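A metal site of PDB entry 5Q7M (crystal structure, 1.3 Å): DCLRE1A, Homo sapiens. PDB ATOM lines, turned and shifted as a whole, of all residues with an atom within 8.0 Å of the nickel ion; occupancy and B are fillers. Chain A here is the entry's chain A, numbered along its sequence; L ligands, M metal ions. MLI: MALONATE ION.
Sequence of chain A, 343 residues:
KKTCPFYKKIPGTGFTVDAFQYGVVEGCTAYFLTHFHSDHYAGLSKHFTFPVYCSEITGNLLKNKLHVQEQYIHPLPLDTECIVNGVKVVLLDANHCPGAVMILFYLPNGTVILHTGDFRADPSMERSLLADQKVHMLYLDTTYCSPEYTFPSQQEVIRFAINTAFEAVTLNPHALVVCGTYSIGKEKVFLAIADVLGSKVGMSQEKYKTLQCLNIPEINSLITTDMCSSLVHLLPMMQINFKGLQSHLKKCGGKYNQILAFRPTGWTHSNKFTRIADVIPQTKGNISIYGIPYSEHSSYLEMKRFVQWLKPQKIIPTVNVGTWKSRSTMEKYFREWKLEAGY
The nickel ion is bound by O8 of the ligand, OD2 of Asp 118, O7 of the ligand, ND1 of His 37, NE2 of His 96 and NE2 of His 35.
The side-chain carboxylate of Asp 118 sits close to a ring nitrogen (NE2) of His 40, at 3.3 Å.
A ring nitrogen (NE2) of His 37 is in hydrogen-bond range of the backbone carbonyl oxygen of Ile 184, 2.9 Å away.
A ring nitrogen (ND1) of His 35 sits at hydrogen-bond distance from the side-chain hydroxyl (OG1) of Thr 34 (2.9 Å).
ND1 of His 96 lies within hydrogen-bond range of O of Glu 296, at 2.8 Å.
Four residues have an atom within 4 Å of the nickel ion: His 35, His 37, His 96 and Asp 118.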
ATOM      1  N   ASP A  18     -13.895  -7.844  25.668  1.00  0.00           N
ATOM      2  CA  ASP A  18     -13.859  -6.363  25.666  1.00  0.00           C
ATOM      3  C   ASP A  18     -15.207  -5.727  26.242  1.00  0.00           C
ATOM      4  O   ASP A  18     -15.745  -4.738  25.720  1.00  0.00           O
ATOM      5  CB  ASP A  18     -13.502  -5.798  24.304  1.00  0.00           C
ATOM      6  CG  ASP A  18     -12.139  -6.309  23.790  1.00  0.00           C
ATOM      7  OD1 ASP A  18     -11.368  -6.863  24.578  1.00  0.00           O
ATOM      8  OD2 ASP A  18     -11.902  -6.092  22.557  1.00  0.00           O
ATOM      9  N   THR A  34      -8.782  -7.970  24.472  1.00  0.00           N
ATOM     10  CA  THR A  34      -7.982  -8.184  23.272  1.00  0.00           C
ATOM     11  C   THR A  34      -6.714  -7.289  23.230  1.00  0.00           C
ATOM     12  O   THR A  34      -5.688  -7.711  22.710  1.00  0.00           O
ATOM     13  CB  THR A  34      -8.780  -8.054  21.958  1.00  0.00           C
ATOM     14  OG1 THR A  34      -9.288  -6.680  21.828  1.00  0.00           O
ATOM     15  CG2 THR A  34      -9.945  -9.079  21.860  1.00  0.00           C
ATOM     16  N   HIS A  35      -6.862  -6.046  23.725  1.00  0.00           N
ATOM     17  CA  HIS A  35      -5.762  -5.034  23.641  1.00  0.00           C
ATOM     18  C   HIS A  35      -6.031  -3.860  24.522  1.00  0.00           C
ATOM     19  O   HIS A  35      -7.210  -3.574  24.854  1.00  0.00           O
ATOM     20  CB  HIS A  35      -5.462  -4.650  22.138  1.00  0.00           C
ATOM     21  CG  HIS A  35      -6.530  -3.840  21.476  1.00  0.00           C
ATOM     22  ND1 HIS A  35      -7.796  -4.320  21.113  1.00  0.00           N
ATOM     23  CD2 HIS A  35      -6.490  -2.561  21.003  1.00  0.00           C
ATOM     24  CE1 HIS A  35      -8.440  -3.351  20.457  1.00  0.00           C
ATOM     25  NE2 HIS A  35      -7.671  -2.304  20.394  1.00  0.00           N
ATOM     26  N   PHE A  36      -4.953  -3.148  24.816  1.00  0.00           N
ATOM     27  CA  PHE A  36      -5.054  -1.960  25.691  1.00  0.00           C
ATOM     28  C   PHE A  36      -5.353  -0.658  24.959  1.00  0.00           C
ATOM     29  O   PHE A  36      -4.450   0.286  24.896  1.00  0.00           O
ATOM     30  CB  PHE A  36      -3.738  -1.866  26.515  1.00  0.00           C
ATOM     31  CG  PHE A  36      -3.800  -0.942  27.734  1.00  0.00           C
ATOM     32  CD1 PHE A  36      -4.430  -1.377  28.893  1.00  0.00           C
ATOM     33  CD2 PHE A  36      -3.189   0.311  27.694  1.00  0.00           C
ATOM     34  CE1 PHE A  36      -4.472  -0.542  30.050  1.00  0.00           C
ATOM     35  CE2 PHE A  36      -3.274   1.166  28.812  1.00  0.00           C
ATOM     36  CZ  PHE A  36      -3.850   0.728  29.969  1.00  0.00           C
ATOM     37  N   HIS A  37      -6.576  -0.557  24.388  1.00  0.00           N
ATOM     38  CA  HIS A  37      -7.134   0.707  23.861  1.00  0.00           C
ATOM     39  C   HIS A  37      -8.392   1.047  24.673  1.00  0.00           C
ATOM     40  O   HIS A  37      -9.190   0.154  24.992  1.00  0.00           O
ATOM     41  CB  HIS A  37      -7.434   0.664  22.351  1.00  0.00           C
ATOM     42  CG  HIS A  37      -6.250   0.858  21.454  1.00  0.00           C
ATOM     43  ND1 HIS A  37      -6.274   0.539  20.106  1.00  0.00           N
ATOM     44  CD2 HIS A  37      -5.048   1.429  21.676  1.00  0.00           C
ATOM     45  CE1 HIS A  37      -5.140   0.905  19.543  1.00  0.00           C
ATOM     46  NE2 HIS A  37      -4.361   1.403  20.509  1.00  0.00           N
ATOM     47  N   SER A  38      -8.602   2.339  24.960  1.00  0.00           N
ATOM     48  CA  SER A  38      -9.618   2.755  25.964  1.00  0.00           C
ATOM     49  C   SER A  38     -11.037   2.329  25.596  1.00  0.00           C
ATOM     50  O   SER A  38     -11.785   1.981  26.537  1.00  0.00           O
ATOM     51  CB  SER A  38      -9.471   4.258  26.291  1.00  0.00           C
ATOM     52  OG  SER A  38      -9.698   5.017  25.145  1.00  0.00           O
ATOM     53  N   ASP A  39     -11.442   2.348  24.331  1.00  0.00           N
ATOM     54  CA  ASP A  39     -12.831   1.927  23.990  1.00  0.00           C
ATOM     55  C   ASP A  39     -13.056   0.453  24.389  1.00  0.00           C
ATOM     56  O   ASP A  39     -14.216  -0.011  24.519  1.00  0.00           O
ATOM     57  CB  ASP A  39     -13.104   2.077  22.494  1.00  0.00           C
ATOM     58  CG  ASP A  39     -13.518   3.565  22.049  1.00  0.00           C
ATOM     59  OD1 ASP A  39     -13.584   4.435  22.921  1.00  0.00           O
ATOM     60  OD2 ASP A  39     -13.686   3.750  20.842  1.00  0.00           O
ATOM     61  N   HIS A  40     -11.951  -0.339  24.459  1.00  0.00           N
ATOM     62  CA  HIS A  40     -12.001  -1.765  24.796  1.00  0.00           C
ATOM     63  C   HIS A  40     -11.798  -2.088  26.238  1.00  0.00           C
ATOM     64  O   HIS A  40     -12.533  -2.979  26.759  1.00  0.00           O
ATOM     65  CB  HIS A  40     -10.941  -2.536  23.887  1.00  0.00           C
ATOM     66  CG  HIS A  40     -11.243  -2.397  22.445  1.00  0.00           C
ATOM     67  ND1 HIS A  40     -11.875  -3.361  21.680  1.00  0.00           N
ATOM     68  CD2 HIS A  40     -10.998  -1.376  21.586  1.00  0.00           C
ATOM     69  CE1 HIS A  40     -12.049  -2.924  20.452  1.00  0.00           C
ATOM     70  NE2 HIS A  40     -11.548  -1.695  20.375  1.00  0.00           N
ATOM     71  N   HIS A  96      -1.933  -5.352  15.262  1.00  0.00           N
ATOM     72  CA  HIS A  96      -2.622  -4.080  15.642  1.00  0.00           C
ATOM     73  C   HIS A  96      -1.593  -3.314  16.419  1.00  0.00           C
ATOM     74  O   HIS A  96      -0.543  -2.958  15.819  1.00  0.00           O
ATOM     75  CB  HIS A  96      -3.964  -4.337  16.316  1.00  0.00           C
ATOM     76  CG  HIS A  96      -4.840  -3.138  16.685  1.00  0.00           C
ATOM     77  ND1 HIS A  96      -5.168  -2.175  15.755  1.00  0.00           N
ATOM     78  CD2 HIS A  96      -5.378  -2.739  17.862  1.00  0.00           C
ATOM     79  CE1 HIS A  96      -5.913  -1.241  16.356  1.00  0.00           C
ATOM     80  NE2 HIS A  96      -6.107  -1.567  17.622  1.00  0.00           N
ATOM     81  N   CYS A  97      -1.814  -2.963  17.669  1.00  0.00           N
ATOM     82  CA  CYS A  97      -0.807  -2.331  18.578  1.00  0.00           C
ATOM     83  C   CYS A  97      -0.068  -3.377  19.413  1.00  0.00           C
ATOM     84  O   CYS A  97      -0.465  -4.558  19.430  1.00  0.00           O
ATOM     85  CB  CYS A  97      -1.559  -1.302  19.482  1.00  0.00           C
ATOM     86  SG  CYS A  97      -2.795  -2.098  20.640  1.00  0.00           S
ATOM     87  N   ALA A 100      -1.714  -6.724  21.247  1.00  0.00           N
ATOM     88  CA  ALA A 100      -3.049  -6.999  20.690  1.00  0.00           C
ATOM     89  C   ALA A 100      -3.157  -8.422  20.158  1.00  0.00           C
ATOM     90  O   ALA A 100      -2.271  -8.849  19.432  1.00  0.00           O
ATOM     91  CB  ALA A 100      -3.417  -6.003  19.635  1.00  0.00           C
ATOM     92  N   GLY A 117     -10.570  -9.288  17.595  1.00  0.00           N
ATOM     93  CA  GLY A 117     -10.341  -8.022  18.276  1.00  0.00           C
ATOM     94  C   GLY A 117     -10.231  -6.934  17.233  1.00  0.00           C
ATOM     95  O   GLY A 117     -10.950  -6.943  16.253  1.00  0.00           O
ATOM     96  N   ASP A 118      -9.337  -5.981  17.452  1.00  0.00           N
ATOM     97  CA  ASP A 118      -8.885  -5.048  16.370  1.00  0.00           C
ATOM     98  C   ASP A 118      -7.677  -5.674  15.622  1.00  0.00           C
ATOM     99  O   ASP A 118      -6.776  -6.202  16.325  1.00  0.00           O
ATOM    100  CB  ASP A 118      -8.524  -3.648  16.910  1.00  0.00           C
ATOM    101  CG  ASP A 118      -9.709  -2.727  17.293  1.00  0.00           C
ATOM    102  OD1 ASP A 118     -10.852  -3.081  16.945  1.00  0.00           O
ATOM    103  OD2 ASP A 118      -9.418  -1.621  17.837  1.00  0.00           O
ATOM    104  N   PHE A 119      -7.675  -5.641  14.311  1.00  0.00           N
ATOM    105  CA  PHE A 119      -6.574  -6.291  13.563  1.00  0.00           C
ATOM    106  C   PHE A 119      -6.259  -5.589  12.238  1.00  0.00           C
ATOM    107  O   PHE A 119      -7.136  -4.913  11.700  1.00  0.00           O
ATOM    108  CB  PHE A 119      -6.784  -7.834  13.368  1.00  0.00           C
ATOM    109  CG  PHE A 119      -7.603  -8.341  12.172  1.00  0.00           C
ATOM    110  CD1 PHE A 119      -7.259  -9.492  11.476  1.00  0.00           C
ATOM    111  CD2 PHE A 119      -8.804  -7.699  11.782  1.00  0.00           C
ATOM    112  CE1 PHE A 119      -8.033  -9.997  10.469  1.00  0.00           C
ATOM    113  CE2 PHE A 119      -9.577  -8.198  10.733  1.00  0.00           C
ATOM    114  CZ  PHE A 119      -9.181  -9.350  10.089  1.00  0.00           C
ATOM    115  N   ASP A 141     -13.369  -7.297  12.990  1.00  0.00           N
ATOM    116  CA  ASP A 141     -13.079  -5.849  12.985  1.00  0.00           C
ATOM    117  C   ASP A 141     -13.319  -5.316  11.602  1.00  0.00           C
ATOM    118  O   ASP A 141     -12.541  -5.472  10.650  1.00  0.00           O
ATOM    119  CB  ASP A 141     -11.627  -5.593  13.391  1.00  0.00           C
ATOM    120  CG  ASP A 141     -11.139  -4.196  13.131  1.00  0.00           C
ATOM    121  OD1 ASP A 141     -12.015  -3.278  12.927  1.00  0.00           O
ATOM    122  OD2 ASP A 141      -9.918  -3.952  13.206  1.00  0.00           O
ATOM    123  N   THR A 143     -13.825  -2.019  10.830  1.00  0.00           N
ATOM    124  CA  THR A 143     -13.563  -0.580  10.812  1.00  0.00           C
ATOM    125  C   THR A 143     -13.608   0.044   9.453  1.00  0.00           C
ATOM    126  O   THR A 143     -14.331   1.069   9.209  1.00  0.00           O
ATOM    127  CB  THR A 143     -12.207  -0.224  11.535  1.00  0.00           C
ATOM    128  OG1 THR A 143     -12.263  -0.609  12.911  1.00  0.00           O
ATOM    129  CG2 THR A 143     -11.890   1.292  11.511  1.00  0.00           C
ATOM    130  N   SER A 183      -2.392   7.093  22.435  1.00  0.00           N
ATOM    131  CA  SER A 183      -2.663   5.721  22.807  1.00  0.00           C
ATOM    132  C   SER A 183      -1.404   4.906  22.433  1.00  0.00           C
ATOM    133  O   SER A 183      -0.569   5.395  21.623  1.00  0.00           O
ATOM    134  CB  SER A 183      -3.837   5.108  21.996  1.00  0.00           C
ATOM    135  OG  SER A 183      -3.606   5.206  20.613  1.00  0.00           O
ATOM    136  N   ILE A 184      -1.271   3.684  22.856  1.00  0.00           N
ATOM    137  CA  ILE A 184      -0.262   2.809  22.304  1.00  0.00           C
ATOM    138  C   ILE A 184      -0.590   2.416  20.878  1.00  0.00           C
ATOM    139  O   ILE A 184      -1.754   2.604  20.388  1.00  0.00           O
ATOM    140  CB  ILE A 184      -0.080   1.512  23.152  1.00  0.00           C
ATOM    141  CG1 ILE A 184      -1.295   0.565  23.132  1.00  0.00           C
ATOM    142  CG2 ILE A 184       0.436   1.819  24.567  1.00  0.00           C
ATOM    143  CD1 ILE A 184      -0.989  -0.829  23.654  1.00  0.00           C
ATOM    144  N   GLU A 296      -3.271   0.812  11.605  1.00  0.00           N
ATOM    145  CA  GLU A 296      -3.219  -0.473  12.326  1.00  0.00           C
ATOM    146  C   GLU A 296      -4.546  -1.283  12.224  1.00  0.00           C
ATOM    147  O   GLU A 296      -4.793  -2.208  13.009  1.00  0.00           O
ATOM    148  CB  GLU A 296      -2.719  -0.314  13.755  1.00  0.00           C
ATOM    149  CG  GLU A 296      -1.183   0.083  13.804  1.00  0.00           C
ATOM    150  CD  GLU A 296      -0.533   0.114  15.162  1.00  0.00           C
ATOM    151  OE1 GLU A 296      -1.253   0.226  16.204  1.00  0.00           O
ATOM    152  OE2 GLU A 296       0.753   0.086  15.207  1.00  0.00           O
ATOM    153  N   HIS A 297      -5.373  -0.881  11.244  1.00  0.00           N
ATOM    154  CA  HIS A 297      -6.536  -1.704  10.859  1.00  0.00           C
ATOM    155  C   HIS A 297      -6.465  -2.128   9.396  1.00  0.00           C
ATOM    156  O   HIS A 297      -5.870  -1.438   8.529  1.00  0.00           O
ATOM    157  CB  HIS A 297      -7.908  -0.901  11.035  1.00  0.00           C
ATOM    158  CG  HIS A 297      -8.228  -0.528  12.435  1.00  0.00           C
ATOM    159  ND1 HIS A 297      -8.903  -1.344  13.318  1.00  0.00           N
ATOM    160  CD2 HIS A 297      -8.010   0.667  13.109  1.00  0.00           C
ATOM    161  CE1 HIS A 297      -9.097  -0.668  14.467  1.00  0.00           C
ATOM    162  NE2 HIS A 297      -8.515   0.497  14.351  1.00  0.00           N
HETATM  163  C1  MLI L   1      -8.729   2.560  18.675  1.00  0.00           C
HETATM  164  C2  MLI L   1      -8.353   2.006  17.298  1.00  0.00           C
HETATM  165  C3  MLI L   1      -9.682   1.590  19.450  1.00  0.00           C
HETATM  166  O6  MLI L   1      -8.516   2.590  16.206  1.00  0.00           O
HETATM  167  O7  MLI L   1      -7.836   0.919  17.303  1.00  0.00           O
HETATM  168  O8  MLI L   1      -9.360   0.420  19.705  1.00  0.00           O
HETATM  169  O9  MLI L   1     -10.777   2.079  19.934  1.00  0.00           O
HETATM  170 NI    NI M   1      -7.766  -0.627  18.861  1.00  0.00          NI
